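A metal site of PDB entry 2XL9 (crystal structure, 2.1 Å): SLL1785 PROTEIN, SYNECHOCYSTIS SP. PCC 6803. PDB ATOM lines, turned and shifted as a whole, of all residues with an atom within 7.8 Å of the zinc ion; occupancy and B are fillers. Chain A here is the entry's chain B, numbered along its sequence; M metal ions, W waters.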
ATOM      1  N   PRO A  56     -10.456 -17.231   3.864  1.00  0.00           N
ATOM      2  CA  PRO A  56      -9.342 -16.746   3.031  1.00  0.00           C
ATOM      3  C   PRO A  56      -9.546 -15.334   2.521  1.00  0.00           C
ATOM      4  O   PRO A  56     -10.678 -14.935   2.232  1.00  0.00           O
ATOM      5  CB  PRO A  56      -9.358 -17.718   1.844  1.00  0.00           C
ATOM      6  CG  PRO A  56     -10.801 -18.025   1.678  1.00  0.00           C
ATOM      7  CD  PRO A  56     -11.317 -18.151   3.097  1.00  0.00           C
ATOM      8  N   MET A  57      -8.433 -14.625   2.353  1.00  0.00           N
ATOM      9  CA  MET A  57      -8.408 -13.320   1.709  1.00  0.00           C
ATOM     10  C   MET A  57      -8.903 -13.513   0.265  1.00  0.00           C
ATOM     11  O   MET A  57      -8.786 -14.612  -0.291  1.00  0.00           O
ATOM     12  CB  MET A  57      -6.956 -12.760   1.720  1.00  0.00           C
ATOM     13  CG  MET A  57      -6.257 -12.484   3.103  1.00  0.00           C
ATOM     14  SD  MET A  57      -7.322 -11.296   4.228  1.00  0.00           S
ATOM     15  CE  MET A  57      -8.379 -12.649   5.169  1.00  0.00           C
ATOM     16  N   PRO A  58      -9.441 -12.444  -0.351  1.00  0.00           N
ATOM     17  CA  PRO A  58      -9.930 -12.505  -1.741  1.00  0.00           C
ATOM     18  C   PRO A  58      -8.943 -13.150  -2.733  1.00  0.00           C
ATOM     19  O   PRO A  58      -7.720 -12.919  -2.659  1.00  0.00           O
ATOM     20  CB  PRO A  58     -10.200 -11.024  -2.086  1.00  0.00           C
ATOM     21  CG  PRO A  58     -10.531 -10.405  -0.734  1.00  0.00           C
ATOM     22  CD  PRO A  58      -9.544 -11.072   0.202  1.00  0.00           C
ATOM     23  N   HIS A  59      -9.454 -13.967  -3.640  1.00  0.00           N
ATOM     24  CA  HIS A  59      -8.605 -14.683  -4.579  1.00  0.00           C
ATOM     25  C   HIS A  59      -9.386 -15.059  -5.843  1.00  0.00           C
ATOM     26  O   HIS A  59     -10.617 -14.941  -5.881  1.00  0.00           O
ATOM     27  CB  HIS A  59      -7.983 -15.932  -3.927  1.00  0.00           C
ATOM     28  CG  HIS A  59      -9.007 -16.928  -3.458  1.00  0.00           C
ATOM     29  ND1 HIS A  59      -9.533 -16.923  -2.191  1.00  0.00           N
ATOM     30  CD2 HIS A  59      -9.604 -17.959  -4.103  1.00  0.00           C
ATOM     31  CE1 HIS A  59     -10.400 -17.914  -2.067  1.00  0.00           C
ATOM     32  NE2 HIS A  59     -10.464 -18.554  -3.217  1.00  0.00           N
ATOM     33  N   ILE A  60      -8.657 -15.512  -6.842  1.00  0.00           N
ATOM     34  CA  ILE A  60      -9.234 -15.866  -8.158  1.00  0.00           C
ATOM     35  C   ILE A  60      -8.726 -17.239  -8.569  1.00  0.00           C
ATOM     36  O   ILE A  60      -7.519 -17.518  -8.467  1.00  0.00           O
ATOM     37  CB  ILE A  60      -8.828 -14.803  -9.239  1.00  0.00           C
ATOM     38  CG1 ILE A  60      -9.203 -13.390  -8.767  1.00  0.00           C
ATOM     39  CG2 ILE A  60      -9.447 -15.145 -10.611  1.00  0.00           C
ATOM     40  CD1 ILE A  60      -8.587 -12.268  -9.581  1.00  0.00           C
ATOM     41  N   HIS A  61      -9.641 -18.099  -9.034  1.00  0.00           N
ATOM     42  CA  HIS A  61      -9.289 -19.437  -9.557  1.00  0.00           C
ATOM     43  C   HIS A  61      -9.150 -19.528 -11.074  1.00  0.00           C
ATOM     44  O   HIS A  61      -9.917 -18.904 -11.812  1.00  0.00           O
ATOM     45  CB  HIS A  61     -10.314 -20.481  -9.124  1.00  0.00           C
ATOM     46  CG  HIS A  61     -10.339 -20.704  -7.658  1.00  0.00           C
ATOM     47  ND1 HIS A  61      -9.436 -21.525  -7.012  1.00  0.00           N
ATOM     48  CD2 HIS A  61     -11.152 -20.209  -6.695  1.00  0.00           C
ATOM     49  CE1 HIS A  61      -9.692 -21.532  -5.721  1.00  0.00           C
ATOM     50  NE2 HIS A  61     -10.726 -20.735  -5.502  1.00  0.00           N
ATOM     51  N   ILE A  64     -10.158 -24.386 -11.485  1.00  0.00           N
ATOM     52  CA  ILE A  64     -11.414 -24.956 -10.952  1.00  0.00           C
ATOM     53  C   ILE A  64     -12.624 -23.999 -11.031  1.00  0.00           C
ATOM     54  O   ILE A  64     -12.466 -22.800 -11.228  1.00  0.00           O
ATOM     55  CB  ILE A  64     -11.251 -25.538  -9.474  1.00  0.00           C
ATOM     56  CG1 ILE A  64     -10.948 -24.460  -8.447  1.00  0.00           C
ATOM     57  CG2 ILE A  64     -10.174 -26.596  -9.418  1.00  0.00           C
ATOM     58  CD1 ILE A  64     -12.157 -23.849  -7.812  1.00  0.00           C
ATOM     59  N   ASN A  65     -13.813 -24.579 -10.895  1.00  0.00           N
ATOM     60  CA  ASN A  65     -15.064 -23.876 -10.598  1.00  0.00           C
ATOM     61  C   ASN A  65     -15.481 -24.290  -9.188  1.00  0.00           C
ATOM     62  O   ASN A  65     -15.316 -25.469  -8.805  1.00  0.00           O
ATOM     63  CB  ASN A  65     -16.171 -24.288 -11.580  1.00  0.00           C
ATOM     64  CG  ASN A  65     -15.872 -23.862 -13.026  1.00  0.00           C
ATOM     65  OD1 ASN A  65     -15.691 -22.693 -13.316  1.00  0.00           O
ATOM     66  ND2 ASN A  65     -15.862 -24.834 -13.936  1.00  0.00           N
ATOM     67  N   GLU A  66     -16.024 -23.346  -8.411  1.00  0.00           N
ATOM     68  CA  GLU A  66     -16.181 -23.547  -6.984  1.00  0.00           C
ATOM     69  C   GLU A  66     -17.656 -23.460  -6.565  1.00  0.00           C
ATOM     70  O   GLU A  66     -18.415 -22.624  -7.061  1.00  0.00           O
ATOM     71  CB  GLU A  66     -15.302 -22.559  -6.188  1.00  0.00           C
ATOM     72  CG  GLU A  66     -15.236 -22.859  -4.665  1.00  0.00           C
ATOM     73  CD  GLU A  66     -14.097 -22.163  -3.940  1.00  0.00           C
ATOM     74  OE1 GLU A  66     -13.286 -21.447  -4.574  1.00  0.00           O
ATOM     75  OE2 GLU A  66     -13.983 -22.357  -2.703  1.00  0.00           O
ATOM     76  N   TRP A  67     -18.062 -24.343  -5.659  1.00  0.00           N
ATOM     77  CA  TRP A  67     -19.360 -24.234  -4.996  1.00  0.00           C
ATOM     78  C   TRP A  67     -19.131 -24.018  -3.506  1.00  0.00           C
ATOM     79  O   TRP A  67     -18.224 -24.625  -2.923  1.00  0.00           O
ATOM     80  CB  TRP A  67     -20.177 -25.523  -5.179  1.00  0.00           C
ATOM     81  CG  TRP A  67     -20.784 -25.761  -6.544  1.00  0.00           C
ATOM     82  CD1 TRP A  67     -22.109 -25.648  -6.888  1.00  0.00           C
ATOM     83  CD2 TRP A  67     -20.112 -26.217  -7.733  1.00  0.00           C
ATOM     84  NE1 TRP A  67     -22.296 -26.005  -8.209  1.00  0.00           N
ATOM     85  CE2 TRP A  67     -21.085 -26.338  -8.753  1.00  0.00           C
ATOM     86  CE3 TRP A  67     -18.766 -26.507  -8.036  1.00  0.00           C
ATOM     87  CZ2 TRP A  67     -20.762 -26.762 -10.055  1.00  0.00           C
ATOM     88  CZ3 TRP A  67     -18.452 -26.919  -9.325  1.00  0.00           C
ATOM     89  CH2 TRP A  67     -19.434 -27.036 -10.325  1.00  0.00           C
ATOM     90  N   PHE A  68     -19.957 -23.168  -2.880  1.00  0.00           N
ATOM     91  CA  PHE A  68     -19.938 -22.954  -1.434  1.00  0.00           C
ATOM     92  C   PHE A  68     -21.301 -23.339  -0.914  1.00  0.00           C
ATOM     93  O   PHE A  68     -22.328 -22.864  -1.452  1.00  0.00           O
ATOM     94  CB  PHE A  68     -19.746 -21.466  -1.074  1.00  0.00           C
ATOM     95  CG  PHE A  68     -18.499 -20.823  -1.602  1.00  0.00           C
ATOM     96  CD1 PHE A  68     -17.355 -20.757  -0.803  1.00  0.00           C
ATOM     97  CD2 PHE A  68     -18.468 -20.242  -2.862  1.00  0.00           C
ATOM     98  CE1 PHE A  68     -16.185 -20.144  -1.270  1.00  0.00           C
ATOM     99  CE2 PHE A  68     -17.299 -19.615  -3.342  1.00  0.00           C
ATOM    100  CZ  PHE A  68     -16.167 -19.570  -2.549  1.00  0.00           C
ATOM    101  N   SER A 114     -19.493 -20.228  -7.915  1.00  0.00           N
ATOM    102  CA  SER A 114     -18.507 -19.269  -8.333  1.00  0.00           C
ATOM    103  C   SER A 114     -17.558 -19.825  -9.416  1.00  0.00           C
ATOM    104  O   SER A 114     -16.553 -20.472  -9.091  1.00  0.00           O
ATOM    105  CB  SER A 114     -17.725 -18.765  -7.122  1.00  0.00           C
ATOM    106  OG  SER A 114     -16.997 -17.612  -7.488  1.00  0.00           O
ATOM    107  N   TYR A 118     -13.790 -15.305 -11.471  1.00  0.00           N
ATOM    108  CA  TYR A 118     -14.377 -14.292 -10.588  1.00  0.00           C
ATOM    109  C   TYR A 118     -13.530 -14.180  -9.333  1.00  0.00           C
ATOM    110  O   TYR A 118     -12.911 -15.158  -8.920  1.00  0.00           O
ATOM    111  CB  TYR A 118     -15.771 -14.691 -10.154  1.00  0.00           C
ATOM    112  CG  TYR A 118     -16.826 -14.534 -11.205  1.00  0.00           C
ATOM    113  CD1 TYR A 118     -17.536 -13.336 -11.331  1.00  0.00           C
ATOM    114  CD2 TYR A 118     -17.168 -15.594 -12.049  1.00  0.00           C
ATOM    115  CE1 TYR A 118     -18.526 -13.180 -12.273  1.00  0.00           C
ATOM    116  CE2 TYR A 118     -18.184 -15.451 -13.030  1.00  0.00           C
ATOM    117  CZ  TYR A 118     -18.846 -14.240 -13.118  1.00  0.00           C
ATOM    118  OH  TYR A 118     -19.845 -14.073 -14.047  1.00  0.00           O
ATOM    119  N   MET A 119     -13.504 -12.992  -8.738  1.00  0.00           N
ATOM    120  CA  MET A 119     -12.872 -12.806  -7.446  1.00  0.00           C
ATOM    121  C   MET A 119     -13.862 -13.145  -6.334  1.00  0.00           C
ATOM    122  O   MET A 119     -15.016 -12.691  -6.370  1.00  0.00           O
ATOM    123  CB  MET A 119     -12.388 -11.363  -7.275  1.00  0.00           C
ATOM    124  CG  MET A 119     -11.525 -11.153  -6.049  1.00  0.00           C
ATOM    125  SD  MET A 119     -11.039  -9.310  -5.803  1.00  0.00           S
ATOM    126  CE  MET A 119     -10.074  -8.960  -7.458  1.00  0.00           C
ATOM    127  N   HIS A 120     -13.414 -13.917  -5.362  1.00  0.00           N
ATOM    128  CA  HIS A 120     -14.229 -14.267  -4.219  1.00  0.00           C
ATOM    129  C   HIS A 120     -13.398 -14.459  -2.951  1.00  0.00           C
ATOM    130  O   HIS A 120     -12.149 -14.502  -2.981  1.00  0.00           O
ATOM    131  CB  HIS A 120     -15.132 -15.471  -4.510  1.00  0.00           C
ATOM    132  CG  HIS A 120     -14.423 -16.789  -4.688  1.00  0.00           C
ATOM    133  ND1 HIS A 120     -14.807 -17.708  -5.641  1.00  0.00           N
ATOM    134  CD2 HIS A 120     -13.366 -17.349  -4.038  1.00  0.00           C
ATOM    135  CE1 HIS A 120     -14.017 -18.768  -5.578  1.00  0.00           C
ATOM    136  NE2 HIS A 120     -13.147 -18.582  -4.599  1.00  0.00           N
ATOM    137  N   GLY A 121     -14.120 -14.567  -1.833  1.00  0.00           N
ATOM    138  CA  GLY A 121     -13.563 -14.877  -0.523  1.00  0.00           C
ATOM    139  C   GLY A 121     -14.726 -14.998   0.440  1.00  0.00           C
ATOM    140  O   GLY A 121     -15.902 -14.841   0.044  1.00  0.00           O
ATOM    141  N   PHE A 122     -14.424 -15.260   1.706  1.00  0.00           N
ATOM    142  CA  PHE A 122     -15.446 -15.261   2.741  1.00  0.00           C
ATOM    143  C   PHE A 122     -14.798 -15.098   4.111  1.00  0.00           C
ATOM    144  O   PHE A 122     -13.573 -15.285   4.281  1.00  0.00           O
ATOM    145  CB  PHE A 122     -16.282 -16.571   2.698  1.00  0.00           C
ATOM    146  CG  PHE A 122     -15.539 -17.772   3.215  1.00  0.00           C
ATOM    147  CD1 PHE A 122     -14.805 -18.564   2.336  1.00  0.00           C
ATOM    148  CD2 PHE A 122     -15.529 -18.082   4.585  1.00  0.00           C
ATOM    149  CE1 PHE A 122     -14.074 -19.672   2.807  1.00  0.00           C
ATOM    150  CE2 PHE A 122     -14.815 -19.189   5.073  1.00  0.00           C
ATOM    151  CZ  PHE A 122     -14.090 -19.984   4.191  1.00  0.00           C
ATOM    152  N   PHE A 134     -16.981 -26.856   0.676  1.00  0.00           N
ATOM    153  CA  PHE A 134     -16.446 -26.453  -0.609  1.00  0.00           C
ATOM    154  C   PHE A 134     -16.409 -27.644  -1.565  1.00  0.00           C
ATOM    155  O   PHE A 134     -16.059 -28.763  -1.162  1.00  0.00           O
ATOM    156  CB  PHE A 134     -15.021 -25.926  -0.483  1.00  0.00           C
ATOM    157  CG  PHE A 134     -14.849 -24.892   0.580  1.00  0.00           C
ATOM    158  CD1 PHE A 134     -14.358 -25.245   1.836  1.00  0.00           C
ATOM    159  CD2 PHE A 134     -15.189 -23.561   0.347  1.00  0.00           C
ATOM    160  CE1 PHE A 134     -14.203 -24.304   2.831  1.00  0.00           C
ATOM    161  CE2 PHE A 134     -15.040 -22.599   1.335  1.00  0.00           C
ATOM    162  CZ  PHE A 134     -14.547 -22.974   2.581  1.00  0.00           C
ATOM    163  N   TRP A 136     -14.567 -28.071  -5.372  1.00  0.00           N
ATOM    164  CA  TRP A 136     -13.709 -27.456  -6.368  1.00  0.00           C
ATOM    165  C   TRP A 136     -13.551 -28.418  -7.544  1.00  0.00           C
ATOM    166  O   TRP A 136     -12.806 -29.397  -7.449  1.00  0.00           O
ATOM    167  CB  TRP A 136     -12.326 -27.183  -5.807  1.00  0.00           C
ATOM    168  CG  TRP A 136     -12.225 -26.268  -4.600  1.00  0.00           C
ATOM    169  CD1 TRP A 136     -12.263 -24.909  -4.594  1.00  0.00           C
ATOM    170  CD2 TRP A 136     -11.994 -26.664  -3.237  1.00  0.00           C
ATOM    171  NE1 TRP A 136     -12.102 -24.426  -3.312  1.00  0.00           N
ATOM    172  CE2 TRP A 136     -11.929 -25.480  -2.459  1.00  0.00           C
ATOM    173  CE3 TRP A 136     -11.857 -27.911  -2.603  1.00  0.00           C
ATOM    174  CZ2 TRP A 136     -11.722 -25.503  -1.077  1.00  0.00           C
ATOM    175  CZ3 TRP A 136     -11.645 -27.924  -1.211  1.00  0.00           C
ATOM    176  CH2 TRP A 136     -11.581 -26.734  -0.470  1.00  0.00           C
ATOM    177  N   MET A 152      -6.694 -28.290  -6.190  1.00  0.00           N
ATOM    178  CA  MET A 152      -7.020 -27.677  -4.875  1.00  0.00           C
ATOM    179  C   MET A 152      -6.560 -28.462  -3.640  1.00  0.00           C
ATOM    180  O   MET A 152      -6.080 -27.855  -2.691  1.00  0.00           O
ATOM    181  CB  MET A 152      -8.508 -27.318  -4.765  1.00  0.00           C
ATOM    182  CG  MET A 152      -8.921 -26.149  -5.681  1.00  0.00           C
ATOM    183  SD  MET A 152      -7.738 -24.590  -5.561  1.00  0.00           S
ATOM    184  CE  MET A 152      -8.098 -24.043  -3.697  1.00  0.00           C
ATOM    185  N   PHE A 156      -3.805 -27.281  -0.706  1.00  0.00           N
ATOM    186  CA  PHE A 156      -3.993 -27.273   0.756  1.00  0.00           C
ATOM    187  C   PHE A 156      -3.023 -28.203   1.471  1.00  0.00           C
ATOM    188  O   PHE A 156      -2.507 -27.862   2.528  1.00  0.00           O
ATOM    189  CB  PHE A 156      -5.444 -27.558   1.156  1.00  0.00           C
ATOM    190  CG  PHE A 156      -6.380 -26.441   0.800  1.00  0.00           C
ATOM    191  CD1 PHE A 156      -6.303 -25.208   1.454  1.00  0.00           C
ATOM    192  CD2 PHE A 156      -7.307 -26.597  -0.216  1.00  0.00           C
ATOM    193  CE1 PHE A 156      -7.168 -24.153   1.099  1.00  0.00           C
ATOM    194  CE2 PHE A 156      -8.166 -25.562  -0.564  1.00  0.00           C
ATOM    195  CZ  PHE A 156      -8.098 -24.326   0.080  1.00  0.00           C
ATOM    196  N   ILE A 189      -4.253 -20.330  -8.591  1.00  0.00           N
ATOM    197  CA  ILE A 189      -4.919 -19.351  -7.736  1.00  0.00           C
ATOM    198  C   ILE A 189      -4.076 -18.083  -7.666  1.00  0.00           C
ATOM    199  O   ILE A 189      -2.878 -18.135  -7.452  1.00  0.00           O
ATOM    200  CB  ILE A 189      -5.126 -19.877  -6.272  1.00  0.00           C
ATOM    201  CG1 ILE A 189      -5.611 -21.333  -6.267  1.00  0.00           C
ATOM    202  CG2 ILE A 189      -6.110 -18.982  -5.513  1.00  0.00           C
ATOM    203  CD1 ILE A 189      -5.213 -22.113  -4.991  1.00  0.00           C
ATOM    204  N   GLN A 191      -3.827 -15.551  -5.047  1.00  0.00           N
ATOM    205  CA  GLN A 191      -4.274 -15.352  -3.652  1.00  0.00           C
ATOM    206  C   GLN A 191      -3.669 -14.104  -3.025  1.00  0.00           C
ATOM    207  O   GLN A 191      -2.444 -14.024  -2.878  1.00  0.00           O
ATOM    208  CB  GLN A 191      -3.933 -16.589  -2.804  1.00  0.00           C
ATOM    209  CG  GLN A 191      -4.207 -16.417  -1.320  1.00  0.00           C
ATOM    210  CD  GLN A 191      -5.689 -16.312  -1.028  1.00  0.00           C
ATOM    211  OE1 GLN A 191      -6.424 -17.270  -1.247  1.00  0.00           O
ATOM    212  NE2 GLN A 191      -6.141 -15.167  -0.513  1.00  0.00           N
HETATM  213 ZN    ZN M   1     -11.904 -20.057  -3.859  1.00  0.00          ZN
HETATM  214  O   HOH W   1     -12.933 -20.735  -1.492  1.00  0.00           O
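The nearest printed residue that does not touch the zinc ion is Trp 136 (4.4 Å).
OG of Ser 114 lies within hydrogen-bond range of ND1 of His 120, at 2.9 Å. The indole nitrogen (NE1) of Trp 136 lies within hydrogen-bond range of the side-chain carboxylate (OE2) of Glu 66. N of Ser 114 is in hydrogen-bond range of O of Glu 66 (2.8 Å). A ring nitrogen (ND1) of His 61 sits close to the side-chain sulfur of Met 152, 3.8 Å away. OE1 of Gln 191 is in hydrogen-bond range of ND1 of His 59, at 3.3 Å. A ring nitrogen (ND1) of His 59 is in hydrogen-bond range of the backbone carbonyl oxygen of Met 57, 3.1 Å away.
The zinc ion is bound by NE2 of His 120, at 2.1 Å. OE1 of Glu 66 is bound to the zinc ion (2.1 Å). NE2 of His 61 is bound to the zinc ion (2.1 Å). The zinc ion is bound by a ring nitrogen (NE2) of His 59. Slightly farther from the zinc ion lies water W1 (2.7 Å).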
